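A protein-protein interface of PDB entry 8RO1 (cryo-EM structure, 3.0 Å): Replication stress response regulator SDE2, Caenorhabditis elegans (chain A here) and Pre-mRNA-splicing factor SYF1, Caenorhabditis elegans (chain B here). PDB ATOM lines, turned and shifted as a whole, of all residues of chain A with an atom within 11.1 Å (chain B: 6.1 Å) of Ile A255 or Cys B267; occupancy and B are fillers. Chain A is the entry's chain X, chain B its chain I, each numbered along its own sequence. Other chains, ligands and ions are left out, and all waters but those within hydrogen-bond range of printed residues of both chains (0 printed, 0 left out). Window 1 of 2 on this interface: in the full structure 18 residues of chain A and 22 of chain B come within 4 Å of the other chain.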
ATOM      1  N   GLN A 246     -28.437   9.640  -0.493  1.00  0.00           N
ATOM      2  CA  GLN A 246     -29.131   8.795  -1.461  1.00  0.00           C
ATOM      3  C   GLN A 246     -29.907   9.616  -2.486  1.00  0.00           C
ATOM      4  O   GLN A 246     -30.119   9.151  -3.612  1.00  0.00           O
ATOM      5  CB  GLN A 246     -30.072   7.821  -0.738  1.00  0.00           C
ATOM      6  CG  GLN A 246     -31.422   8.382  -0.242  1.00  0.00           C
ATOM      7  CD  GLN A 246     -31.287   9.546   0.718  1.00  0.00           C
ATOM      8  OE1 GLN A 246     -31.709  10.664   0.419  1.00  0.00           O
ATOM      9  NE2 GLN A 246     -30.686   9.291   1.875  1.00  0.00           N
ATOM     10  N   ASP A 247     -30.338  10.827  -2.125  1.00  0.00           N
ATOM     11  CA  ASP A 247     -31.034  11.677  -3.086  1.00  0.00           C
ATOM     12  C   ASP A 247     -30.083  12.278  -4.114  1.00  0.00           C
ATOM     13  O   ASP A 247     -30.500  12.567  -5.240  1.00  0.00           O
ATOM     14  CB  ASP A 247     -31.868  12.727  -2.318  1.00  0.00           C
ATOM     15  CG  ASP A 247     -31.076  13.963  -1.837  1.00  0.00           C
ATOM     16  OD1 ASP A 247     -30.329  14.639  -2.577  1.00  0.00           O
ATOM     17  OD2 ASP A 247     -31.223  14.270  -0.637  1.00  0.00           O
ATOM     18  N   TYR A 248     -28.809  12.459  -3.762  1.00  0.00           N
ATOM     19  CA  TYR A 248     -27.812  12.777  -4.777  1.00  0.00           C
ATOM     20  C   TYR A 248     -27.595  11.594  -5.707  1.00  0.00           C
ATOM     21  O   TYR A 248     -27.559  11.753  -6.932  1.00  0.00           O
ATOM     22  CB  TYR A 248     -26.491  13.174  -4.118  1.00  0.00           C
ATOM     23  CG  TYR A 248     -25.360  13.410  -5.096  1.00  0.00           C
ATOM     24  CD1 TYR A 248     -25.190  14.636  -5.703  1.00  0.00           C
ATOM     25  CD2 TYR A 248     -24.432  12.416  -5.369  1.00  0.00           C
ATOM     26  CE1 TYR A 248     -24.163  14.849  -6.591  1.00  0.00           C
ATOM     27  CE2 TYR A 248     -23.398  12.628  -6.246  1.00  0.00           C
ATOM     28  CZ  TYR A 248     -23.272  13.844  -6.861  1.00  0.00           C
ATOM     29  OH  TYR A 248     -22.230  14.063  -7.727  1.00  0.00           O
ATOM     30  N   LEU A 249     -27.452  10.398  -5.141  1.00  0.00           N
ATOM     31  CA  LEU A 249     -27.318   9.195  -5.952  1.00  0.00           C
ATOM     32  C   LEU A 249     -28.531   8.967  -6.844  1.00  0.00           C
ATOM     33  O   LEU A 249     -28.396   8.415  -7.940  1.00  0.00           O
ATOM     34  CB  LEU A 249     -27.102   7.987  -5.045  1.00  0.00           C
ATOM     35  CG  LEU A 249     -26.494   6.747  -5.701  1.00  0.00           C
ATOM     36  CD1 LEU A 249     -24.988   6.901  -5.812  1.00  0.00           C
ATOM     37  CD2 LEU A 249     -26.848   5.480  -4.937  1.00  0.00           C
ATOM     38  N   SER A 250     -29.719   9.380  -6.403  1.00  0.00           N
ATOM     39  CA  SER A 250     -30.885   9.354  -7.282  1.00  0.00           C
ATOM     40  C   SER A 250     -30.791  10.390  -8.397  1.00  0.00           C
ATOM     41  O   SER A 250     -31.032  10.075  -9.568  1.00  0.00           O
ATOM     42  CB  SER A 250     -32.154   9.580  -6.464  1.00  0.00           C
ATOM     43  OG  SER A 250     -32.285   8.599  -5.453  1.00  0.00           O
ATOM     44  N   ARG A 251     -30.444  11.634  -8.059  1.00  0.00           N
ATOM     45  CA  ARG A 251     -30.244  12.650  -9.090  1.00  0.00           C
ATOM     46  C   ARG A 251     -29.120  12.300 -10.054  1.00  0.00           C
ATOM     47  O   ARG A 251     -29.177  12.689 -11.225  1.00  0.00           O
ATOM     48  CB  ARG A 251     -29.959  14.009  -8.460  1.00  0.00           C
ATOM     49  CG  ARG A 251     -31.200  14.766  -8.038  1.00  0.00           C
ATOM     50  CD  ARG A 251     -30.830  16.124  -7.472  1.00  0.00           C
ATOM     51  NE  ARG A 251     -30.288  16.025  -6.122  1.00  0.00           N
ATOM     52  CZ  ARG A 251     -29.708  17.016  -5.455  1.00  0.00           C
ATOM     53  NH1 ARG A 251     -29.275  16.795  -4.217  1.00  0.00           N
ATOM     54  NH2 ARG A 251     -29.522  18.210  -5.998  1.00  0.00           N
ATOM     55  N   ARG A 252     -28.096  11.582  -9.587  1.00  0.00           N
ATOM     56  CA  ARG A 252     -27.060  11.070 -10.482  1.00  0.00           C
ATOM     57  C   ARG A 252     -27.637  10.245 -11.623  1.00  0.00           C
ATOM     58  O   ARG A 252     -27.153  10.329 -12.756  1.00  0.00           O
ATOM     59  CB  ARG A 252     -26.061  10.243  -9.678  1.00  0.00           C
ATOM     60  CG  ARG A 252     -24.733   9.989 -10.368  1.00  0.00           C
ATOM     61  CD  ARG A 252     -24.080   8.758  -9.770  1.00  0.00           C
ATOM     62  NE  ARG A 252     -24.712   7.534 -10.248  1.00  0.00           N
ATOM     63  CZ  ARG A 252     -24.458   6.312  -9.797  1.00  0.00           C
ATOM     64  NH1 ARG A 252     -25.026   5.269 -10.396  1.00  0.00           N
ATOM     65  NH2 ARG A 252     -23.704   6.107  -8.728  1.00  0.00           N
ATOM     66  N   GLU A 253     -28.658   9.435 -11.347  1.00  0.00           N
ATOM     67  CA  GLU A 253     -29.281   8.629 -12.394  1.00  0.00           C
ATOM     68  C   GLU A 253     -30.336   9.420 -13.160  1.00  0.00           C
ATOM     69  O   GLU A 253     -30.505   9.219 -14.367  1.00  0.00           O
ATOM     70  CB  GLU A 253     -29.896   7.368 -11.788  1.00  0.00           C
ATOM     71  CG  GLU A 253     -28.882   6.385 -11.215  1.00  0.00           C
ATOM     72  CD  GLU A 253     -27.968   5.792 -12.270  1.00  0.00           C
ATOM     73  OE1 GLU A 253     -28.426   4.924 -13.039  1.00  0.00           O
ATOM     74  OE2 GLU A 253     -26.787   6.197 -12.332  1.00  0.00           O
ATOM     75  N   GLU A 254     -31.085  10.275 -12.459  1.00  0.00           N
ATOM     76  CA  GLU A 254     -32.049  11.164 -13.101  1.00  0.00           C
ATOM     77  C   GLU A 254     -31.382  12.003 -14.185  1.00  0.00           C
ATOM     78  O   GLU A 254     -31.785  11.974 -15.352  1.00  0.00           O
ATOM     79  CB  GLU A 254     -32.724  12.059 -12.063  1.00  0.00           C
ATOM     80  CG  GLU A 254     -33.807  12.955 -12.650  1.00  0.00           C
ATOM     81  CD  GLU A 254     -34.641  13.642 -11.589  1.00  0.00           C
ATOM     82  OE1 GLU A 254     -34.264  13.583 -10.400  1.00  0.00           O
ATOM     83  OE2 GLU A 254     -35.676  14.243 -11.948  1.00  0.00           O
ATOM     84  N   ILE A 255     -30.353  12.762 -13.806  1.00  0.00           N
ATOM     85  CA  ILE A 255     -29.855  13.849 -14.641  1.00  0.00           C
ATOM     86  C   ILE A 255     -29.178  13.304 -15.888  1.00  0.00           C
ATOM     87  O   ILE A 255     -29.246  13.924 -16.952  1.00  0.00           O
ATOM     88  CB  ILE A 255     -28.901  14.722 -13.796  1.00  0.00           C
ATOM     89  CG1 ILE A 255     -29.704  15.512 -12.759  1.00  0.00           C
ATOM     90  CG2 ILE A 255     -28.057  15.695 -14.671  1.00  0.00           C
ATOM     91  CD1 ILE A 255     -28.863  16.167 -11.676  1.00  0.00           C
ATOM     92  N   ILE A 256     -28.513  12.154 -15.794  1.00  0.00           N
ATOM     93  CA  ILE A 256     -27.861  11.596 -16.972  1.00  0.00           C
ATOM     94  C   ILE A 256     -28.905  11.033 -17.923  1.00  0.00           C
ATOM     95  O   ILE A 256     -28.900  11.338 -19.120  1.00  0.00           O
ATOM     96  CB  ILE A 256     -26.839  10.518 -16.560  1.00  0.00           C
ATOM     97  CG1 ILE A 256     -25.697  11.106 -15.709  1.00  0.00           C
ATOM     98  CG2 ILE A 256     -26.265   9.817 -17.802  1.00  0.00           C
ATOM     99  CD1 ILE A 256     -24.982  12.327 -16.276  1.00  0.00           C
ATOM    100  N   ASN A 257     -29.821  10.210 -17.409  1.00  0.00           N
ATOM    101  CA  ASN A 257     -30.724   9.498 -18.305  1.00  0.00           C
ATOM    102  C   ASN A 257     -31.742  10.441 -18.936  1.00  0.00           C
ATOM    103  O   ASN A 257     -32.228  10.168 -20.037  1.00  0.00           O
ATOM    104  CB  ASN A 257     -31.423   8.359 -17.567  1.00  0.00           C
ATOM    105  CG  ASN A 257     -32.716   8.785 -16.930  1.00  0.00           C
ATOM    106  OD1 ASN A 257     -33.797   8.350 -17.323  1.00  0.00           O
ATOM    107  ND2 ASN A 257     -32.615   9.648 -15.940  1.00  0.00           N
ATOM    108  N   LYS A 258     -32.064  11.554 -18.269  1.00  0.00           N
ATOM    109  CA  LYS A 258     -33.026  12.505 -18.811  1.00  0.00           C
ATOM    110  C   LYS A 258     -32.383  13.475 -19.794  1.00  0.00           C
ATOM    111  O   LYS A 258     -33.094  14.097 -20.586  1.00  0.00           O
ATOM    112  CB  LYS A 258     -33.739  13.260 -17.682  1.00  0.00           C
ATOM    113  CG  LYS A 258     -33.047  14.505 -17.119  1.00  0.00           C
ATOM    114  CD  LYS A 258     -33.717  15.782 -17.607  1.00  0.00           C
ATOM    115  CE  LYS A 258     -33.150  17.008 -16.919  1.00  0.00           C
ATOM    116  NZ  LYS A 258     -33.974  18.221 -17.183  1.00  0.00           N
ATOM    117  N   THR A 259     -31.064  13.641 -19.737  1.00  0.00           N
ATOM    118  CA  THR A 259     -30.332  14.302 -20.808  1.00  0.00           C
ATOM    119  C   THR A 259     -29.974  13.356 -21.940  1.00  0.00           C
ATOM    120  O   THR A 259     -29.499  13.826 -22.974  1.00  0.00           O
ATOM    121  CB  THR A 259     -29.043  14.934 -20.289  1.00  0.00           C
ATOM    122  OG1 THR A 259     -28.325  13.979 -19.502  1.00  0.00           O
ATOM    123  CG2 THR A 259     -29.346  16.173 -19.466  1.00  0.00           C
ATOM    124  N   GLU A 260     -30.205  12.053 -21.786  1.00  0.00           N
ATOM    125  CA  GLU A 260     -30.026  11.130 -22.899  1.00  0.00           C
ATOM    126  C   GLU A 260     -31.223  11.137 -23.841  1.00  0.00           C
ATOM    127  O   GLU A 260     -31.052  11.241 -25.059  1.00  0.00           O
ATOM    128  CB  GLU A 260     -29.771   9.717 -22.375  1.00  0.00           C
ATOM    129  CG  GLU A 260     -28.424   9.526 -21.693  1.00  0.00           C
ATOM    130  CD  GLU A 260     -27.348   9.031 -22.644  1.00  0.00           C
ATOM    131  OE1 GLU A 260     -27.229   9.582 -23.755  1.00  0.00           O
ATOM    132  OE2 GLU A 260     -26.617   8.088 -22.277  1.00  0.00           O
ATOM    133  N   ASP A 261     -32.443  11.013 -23.307  1.00  0.00           N
ATOM    134  CA  ASP A 261     -33.620  11.194 -24.157  1.00  0.00           C
ATOM    135  C   ASP A 261     -33.658  12.599 -24.753  1.00  0.00           C
ATOM    136  O   ASP A 261     -34.141  12.783 -25.877  1.00  0.00           O
ATOM    137  CB  ASP A 261     -34.910  10.869 -23.398  1.00  0.00           C
ATOM    138  CG  ASP A 261     -35.402  12.011 -22.549  1.00  0.00           C
ATOM    139  OD1 ASP A 261     -34.756  12.300 -21.533  1.00  0.00           O
ATOM    140  OD2 ASP A 261     -36.422  12.632 -22.909  1.00  0.00           O
ATOM    141  N   ALA A 262     -33.211  13.607 -23.991  1.00  0.00           N
ATOM    142  CA  ALA A 262     -33.155  14.974 -24.505  1.00  0.00           C
ATOM    143  C   ALA A 262     -32.337  15.033 -25.788  1.00  0.00           C
ATOM    144  O   ALA A 262     -32.700  15.739 -26.734  1.00  0.00           O
ATOM    145  CB  ALA A 262     -32.569  15.916 -23.461  1.00  0.00           C
ATOM    146  N   CYS A 263     -31.229  14.294 -25.837  1.00  0.00           N
ATOM    147  CA  CYS A 263     -30.504  14.167 -27.094  1.00  0.00           C
ATOM    148  C   CYS A 263     -31.358  13.467 -28.140  1.00  0.00           C
ATOM    149  O   CYS A 263     -31.381  13.876 -29.305  1.00  0.00           O
ATOM    150  CB  CYS A 263     -29.199  13.395 -26.895  1.00  0.00           C
ATOM    151  SG  CYS A 263     -27.932  14.163 -25.873  1.00  0.00           S
ATOM    152  N   VAL B 262     -28.152  23.245  -7.710  1.00  0.00           N
ATOM    153  CA  VAL B 262     -27.436  23.963  -8.760  1.00  0.00           C
ATOM    154  C   VAL B 262     -26.990  23.008  -9.851  1.00  0.00           C
ATOM    155  O   VAL B 262     -27.112  23.302 -11.044  1.00  0.00           O
ATOM    156  CB  VAL B 262     -26.247  24.730  -8.160  1.00  0.00           C
ATOM    157  CG1 VAL B 262     -25.313  25.257  -9.253  1.00  0.00           C
ATOM    158  CG2 VAL B 262     -26.750  25.875  -7.293  1.00  0.00           C
ATOM    159  N   GLY B 263     -26.441  21.864  -9.467  1.00  0.00           N
ATOM    160  CA  GLY B 263     -26.012  20.907 -10.469  1.00  0.00           C
ATOM    161  C   GLY B 263     -27.153  20.369 -11.310  1.00  0.00           C
ATOM    162  O   GLY B 263     -26.983  20.113 -12.500  1.00  0.00           O
ATOM    163  N   PHE B 264     -28.324  20.177 -10.708  1.00  0.00           N
ATOM    164  CA  PHE B 264     -29.491  19.786 -11.497  1.00  0.00           C
ATOM    165  C   PHE B 264     -29.922  20.881 -12.462  1.00  0.00           C
ATOM    166  O   PHE B 264     -30.204  20.609 -13.632  1.00  0.00           O
ATOM    167  CB  PHE B 264     -30.657  19.412 -10.576  1.00  0.00           C
ATOM    168  CG  PHE B 264     -31.953  19.137 -11.304  1.00  0.00           C
ATOM    169  CD1 PHE B 264     -32.250  17.864 -11.736  1.00  0.00           C
ATOM    170  CD2 PHE B 264     -32.906  20.137 -11.486  1.00  0.00           C
ATOM    171  CE1 PHE B 264     -33.436  17.603 -12.392  1.00  0.00           C
ATOM    172  CE2 PHE B 264     -34.089  19.882 -12.142  1.00  0.00           C
ATOM    173  CZ  PHE B 264     -34.356  18.615 -12.596  1.00  0.00           C
ATOM    174  N   LEU B 265     -29.979  22.128 -11.993  1.00  0.00           N
ATOM    175  CA  LEU B 265     -30.521  23.201 -12.823  1.00  0.00           C
ATOM    176  C   LEU B 265     -29.602  23.620 -13.962  1.00  0.00           C
ATOM    177  O   LEU B 265     -30.097  24.036 -15.012  1.00  0.00           O
ATOM    178  CB  LEU B 265     -30.864  24.401 -11.947  1.00  0.00           C
ATOM    179  CG  LEU B 265     -32.047  24.211 -10.993  1.00  0.00           C
ATOM    180  CD1 LEU B 265     -32.207  25.425 -10.135  1.00  0.00           C
ATOM    181  CD2 LEU B 265     -33.336  23.974 -11.753  1.00  0.00           C
ATOM    182  N   TRP B 266     -28.284  23.526 -13.803  1.00  0.00           N
ATOM    183  CA  TRP B 266     -27.413  23.713 -14.964  1.00  0.00           C
ATOM    184  C   TRP B 266     -27.690  22.686 -16.055  1.00  0.00           C
ATOM    185  O   TRP B 266     -27.728  23.032 -17.238  1.00  0.00           O
ATOM    186  CB  TRP B 266     -25.942  23.676 -14.564  1.00  0.00           C
ATOM    187  CG  TRP B 266     -25.449  24.938 -13.933  1.00  0.00           C
ATOM    188  CD1 TRP B 266     -24.960  25.081 -12.680  1.00  0.00           C
ATOM    189  CD2 TRP B 266     -25.359  26.224 -14.548  1.00  0.00           C
ATOM    190  NE1 TRP B 266     -24.594  26.381 -12.461  1.00  0.00           N
ATOM    191  CE2 TRP B 266     -24.826  27.103 -13.597  1.00  0.00           C
ATOM    192  CE3 TRP B 266     -25.683  26.716 -15.808  1.00  0.00           C
ATOM    193  CZ2 TRP B 266     -24.608  28.440 -13.865  1.00  0.00           C
ATOM    194  CZ3 TRP B 266     -25.470  28.048 -16.068  1.00  0.00           C
ATOM    195  CH2 TRP B 266     -24.941  28.893 -15.103  1.00  0.00           C
ATOM    196  N   CYS B 267     -27.893  21.428 -15.689  1.00  0.00           N
ATOM    197  CA  CYS B 267     -28.291  20.445 -16.692  1.00  0.00           C
ATOM    198  C   CYS B 267     -29.685  20.716 -17.236  1.00  0.00           C
ATOM    199  O   CYS B 267     -29.947  20.479 -18.420  1.00  0.00           O
ATOM    200  CB  CYS B 267     -28.207  19.044 -16.111  1.00  0.00           C
ATOM    201  SG  CYS B 267     -26.549  18.609 -15.627  1.00  0.00           S
ATOM    202  N   SER B 268     -30.599  21.188 -16.398  1.00  0.00           N
ATOM    203  CA  SER B 268     -31.938  21.501 -16.883  1.00  0.00           C
ATOM    204  C   SER B 268     -31.926  22.650 -17.877  1.00  0.00           C
ATOM    205  O   SER B 268     -32.724  22.667 -18.816  1.00  0.00           O
ATOM    206  CB  SER B 268     -32.862  21.821 -15.718  1.00  0.00           C
ATOM    207  OG  SER B 268     -34.194  21.946 -16.176  1.00  0.00           O
ATOM    208  N   LEU B 269     -31.068  23.643 -17.667  1.00  0.00           N
ATOM    209  CA  LEU B 269     -30.938  24.701 -18.660  1.00  0.00           C
ATOM    210  C   LEU B 269     -30.367  24.181 -19.967  1.00  0.00           C
ATOM    211  O   LEU B 269     -30.827  24.574 -21.041  1.00  0.00           O
ATOM    212  CB  LEU B 269     -30.059  25.818 -18.113  1.00  0.00           C
ATOM    213  CG  LEU B 269     -29.810  27.038 -18.991  1.00  0.00           C
ATOM    214  CD1 LEU B 269     -31.092  27.712 -19.395  1.00  0.00           C
ATOM    215  CD2 LEU B 269     -28.909  28.001 -18.251  1.00  0.00           C
ATOM    216  N   ALA B 270     -29.370  23.298 -19.907  1.00  0.00           N
ATOM    217  CA  ALA B 270     -28.836  22.718 -21.134  1.00  0.00           C
ATOM    218  C   ALA B 270     -29.863  21.835 -21.829  1.00  0.00           C
ATOM    219  O   ALA B 270     -29.954  21.832 -23.060  1.00  0.00           O
ATOM    220  CB  ALA B 270     -27.572  21.921 -20.834  1.00  0.00           C
ATOM    221  N   ASP B 271     -30.617  21.055 -21.052  1.00  0.00           N
ATOM    222  CA  ASP B 271     -31.698  20.229 -21.584  1.00  0.00           C
ATOM    223  C   ASP B 271     -32.686  21.042 -22.413  1.00  0.00           C
ATOM    224  O   ASP B 271     -33.135  20.595 -23.473  1.00  0.00           O
ATOM    225  CB  ASP B 271     -32.405  19.532 -20.418  1.00  0.00           C
ATOM    226  CG  ASP B 271     -33.564  18.632 -20.853  1.00  0.00           C
ATOM    227  OD1 ASP B 271     -33.747  18.371 -22.062  1.00  0.00           O
ATOM    228  OD2 ASP B 271     -34.314  18.185 -19.958  1.00  0.00           O
ATOM    229  N   TYR B 272     -33.048  22.232 -21.936  1.00  0.00           N
ATOM    230  CA  TYR B 272     -33.891  23.142 -22.707  1.00  0.00           C
ATOM    231  C   TYR B 272     -33.286  23.471 -24.065  1.00  0.00           C
ATOM    232  O   TYR B 272     -33.967  23.402 -25.090  1.00  0.00           O
ATOM    233  CB  TYR B 272     -34.125  24.412 -21.900  1.00  0.00           C
ATOM    234  CG  TYR B 272     -34.597  25.592 -22.689  1.00  0.00           C
ATOM    235  CD1 TYR B 272     -35.907  25.702 -23.076  1.00  0.00           C
ATOM    236  CD2 TYR B 272     -33.747  26.626 -22.994  1.00  0.00           C
ATOM    237  CE1 TYR B 272     -36.353  26.785 -23.775  1.00  0.00           C
ATOM    238  CE2 TYR B 272     -34.189  27.721 -23.694  1.00  0.00           C
ATOM    239  CZ  TYR B 272     -35.491  27.794 -24.083  1.00  0.00           C
ATOM    240  OH  TYR B 272     -35.942  28.884 -24.781  1.00  0.00           O
ATOM    241  N   ILE B 274     -30.896  21.786 -25.683  1.00  0.00           N
ATOM    242  CA  ILE B 274     -30.763  20.572 -26.488  1.00  0.00           C
ATOM    243  C   ILE B 274     -32.092  20.241 -27.161  1.00  0.00           C
ATOM    244  O   ILE B 274     -32.134  19.900 -28.347  1.00  0.00           O
ATOM    245  CB  ILE B 274     -30.243  19.405 -25.625  1.00  0.00           C
ATOM    246  CG1 ILE B 274     -28.804  19.676 -25.180  1.00  0.00           C
ATOM    247  CG2 ILE B 274     -30.246  18.078 -26.408  1.00  0.00           C
ATOM    248  CD1 ILE B 274     -28.331  18.836 -24.002  1.00  0.00           C
ATOM    249  N   VAL B 285     -23.748  26.638 -22.214  1.00  0.00           N
ATOM    250  CA  VAL B 285     -24.261  26.422 -20.866  1.00  0.00           C
ATOM    251  C   VAL B 285     -23.379  25.469 -20.075  1.00  0.00           C
ATOM    252  O   VAL B 285     -23.086  25.716 -18.903  1.00  0.00           O
ATOM    253  CB  VAL B 285     -25.710  25.924 -20.935  1.00  0.00           C
ATOM    254  CG1 VAL B 285     -26.159  25.341 -19.603  1.00  0.00           C
ATOM    255  CG2 VAL B 285     -26.623  27.062 -21.371  1.00  0.00           C
ATOM    256  N   TYR B 286     -22.962  24.359 -20.677  1.00  0.00           N
ATOM    257  CA  TYR B 286     -22.083  23.445 -19.956  1.00  0.00           C
ATOM    258  C   TYR B 286     -20.736  24.091 -19.669  1.00  0.00           C
ATOM    259  O   TYR B 286     -20.211  23.978 -18.558  1.00  0.00           O
ATOM    260  CB  TYR B 286     -21.887  22.148 -20.740  1.00  0.00           C
ATOM    261  CG  TYR B 286     -23.056  21.201 -20.671  1.00  0.00           C
ATOM    262  CD1 TYR B 286     -23.443  20.626 -19.485  1.00  0.00           C
ATOM    263  CD2 TYR B 286     -23.736  20.842 -21.812  1.00  0.00           C
ATOM    264  CE1 TYR B 286     -24.491  19.761 -19.434  1.00  0.00           C
ATOM    265  CE2 TYR B 286     -24.785  19.977 -21.762  1.00  0.00           C
ATOM    266  CZ  TYR B 286     -25.159  19.439 -20.571  1.00  0.00           C
ATOM    267  OH  TYR B 286     -26.214  18.567 -20.521  1.00  0.00           O
ATOM    268  N   GLN B 301     -22.159  16.289 -11.536  1.00  0.00           N
ATOM    269  CA  GLN B 301     -23.373  16.169 -12.333  1.00  0.00           C
ATOM    270  C   GLN B 301     -23.208  16.862 -13.677  1.00  0.00           C
ATOM    271  O   GLN B 301     -23.595  16.319 -14.715  1.00  0.00           O
ATOM    272  CB  GLN B 301     -24.565  16.734 -11.569  1.00  0.00           C
ATOM    273  CG  GLN B 301     -24.856  16.001 -10.273  1.00  0.00           C
ATOM    274  CD  GLN B 301     -25.950  16.657  -9.471  1.00  0.00           C
ATOM    275  OE1 GLN B 301     -26.299  17.808  -9.702  1.00  0.00           O
ATOM    276  NE2 GLN B 301     -26.499  15.925  -8.517  1.00  0.00           N
ATOM    277  N   VAL B 302     -22.664  18.078 -13.667  1.00  0.00           N
ATOM    278  CA  VAL B 302     -22.602  18.876 -14.886  1.00  0.00           C
ATOM    279  C   VAL B 302     -21.654  18.243 -15.893  1.00  0.00           C
ATOM    280  O   VAL B 302     -21.992  18.096 -17.071  1.00  0.00           O
ATOM    281  CB  VAL B 302     -22.210  20.329 -14.573  1.00  0.00           C
ATOM    282  CG1 VAL B 302     -22.104  21.135 -15.860  1.00  0.00           C
ATOM    283  CG2 VAL B 302     -23.237  20.958 -13.622  1.00  0.00           C
ATOM    284  N   ALA B 305     -22.980  14.799 -17.174  1.00  0.00           N
ATOM    285  CA  ALA B 305     -24.008  15.070 -18.167  1.00  0.00           C
ATOM    286  C   ALA B 305     -23.402  15.597 -19.458  1.00  0.00           C
ATOM    287  O   ALA B 305     -23.839  15.230 -20.552  1.00  0.00           O
ATOM    288  CB  ALA B 305     -25.011  16.071 -17.605  1.00  0.00           C
ATOM    289  N   TYR B 306     -22.383  16.446 -19.351  1.00  0.00           N
ATOM    290  CA  TYR B 306     -21.772  17.036 -20.539  1.00  0.00           C
ATOM    291  C   TYR B 306     -21.055  15.991 -21.382  1.00  0.00           C
ATOM    292  O   TYR B 306     -21.196  15.975 -22.607  1.00  0.00           O
ATOM    293  CB  TYR B 306     -20.809  18.146 -20.115  1.00  0.00           C
ATOM    294  CG  TYR B 306     -20.145  18.962 -21.210  1.00  0.00           C
ATOM    295  CD1 TYR B 306     -20.664  19.050 -22.484  1.00  0.00           C
ATOM    296  CD2 TYR B 306     -19.002  19.683 -20.936  1.00  0.00           C
ATOM    297  CE1 TYR B 306     -20.041  19.795 -23.448  1.00  0.00           C
ATOM    298  CE2 TYR B 306     -18.391  20.436 -21.888  1.00  0.00           C
ATOM    299  CZ  TYR B 306     -18.906  20.491 -23.142  1.00  0.00           C
ATOM    300  OH  TYR B 306     -18.286  21.261 -24.097  1.00  0.00           O
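Of the 18 printed residues of chain B, 7 touch a printed residue of chain A.
Printed residues of chain B that touch a printed residue of chain A: Phe B264, Cys B267, Ser B268, Asp B271, Ile B274, Gln B301 and Ala B305.
Printed residues of chain A that touch a printed residue of chain B: Tyr A248, Arg A251, Ile A255, Ile A256, Lys A258, Ala A262 and Cys A263.
Hydrophobic or aromatic side chains of chain A within 4 Å of the printed part of chain B: Tyr A248, Ile A255, Ile A256 and Ala A262.
Gln B301 touches Tyr A248.
Arg A251 touches Gln B301 (CB to NE2, 3.96 Å).
CG1 of Ile A255 touches CD1 of Phe B264, at 3.6 Å.
Cys B267 touches Ile A255.
Gln B301 touches Ile A255 (OE1 to CD1, 3.6 Å).
Ala B305 touches Ile A256 (N to CD1, 3.3 Å).
Lys A258 touches Ser B268.
Ala A262 touches Asp B271 (CB to OD1, 3.1 Å).
O of Ala A262 touches CG2 of Ile B274, 3.4 Å away.
Ile B274 touches Cys A263 (CG2 to N, 3.95 Å).
NZ of Lys A258 lies within salt-bridge range of OD2 of Asp B271, 2.8 Å away.
Of the printed residues of chain B, Tyr A248 touches Gln B301.
Printed residues of chain B within 4 Å of Arg A251: Gln B301 (3.96 Å).
Printed residues of chain B within 4 Å of Ile A256: Ala B305.
Of the printed residues of chain B, Lys A258 touches Ser B268 (3.9 Å) and Asp B271 (2.8 Å).
Of the printed residues of chain B, Ala A262 touches Asp B271 (3.1 Å) and Ile B274 (3.4 Å).
No residue of chain A comes within 4 Å of Gly B263.
Phe B264 touches one residue of chain A.
Of chain A, only Ile A255 comes within 4 Å of Cys B267.
Of the printed residues of chain A, Asp B271 touches Lys A258 and Ala A262.
Val B285 touches none of the printed residues of chain A.
Tyr B286 touches none of the printed residues of chain A.
Printed residues of chain A within 4 Å of Gln B301: Tyr A248, Arg A251 and Ile A255.
No residue of chain A comes within 4 Å of Val B302.
Printed residues of chain A within 4 Å of Ala B305: Ile A256 (3.3 Å).
The nearest printed residue of chain B that does not touch Tyr A248 is Val B302 (7.2 Å).
OD1 of Asp A247 lies within salt-bridge range of NH1 of Arg A251 (2.9 Å).
OE1 of Gln B301 is in hydrogen-bond range of N of Phe B264, at 3.3 Å.
OG1 of Thr A259 sits at hydrogen-bond distance from O of Ile A255, 2.7 Å away.
The side-chain sulfur (SG) of Cys B267 is in hydrogen-bond range of the backbone carbonyl oxygen (O) of Gly B263 (3.5 Å).
The backbone carbonyl oxygen of Thr A259 lies within hydrogen-bond range of the side-chain sulfur of Cys A263 (3.3 Å).
O of Ile A256 sits at hydrogen-bond distance from OG1 of Thr A259.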
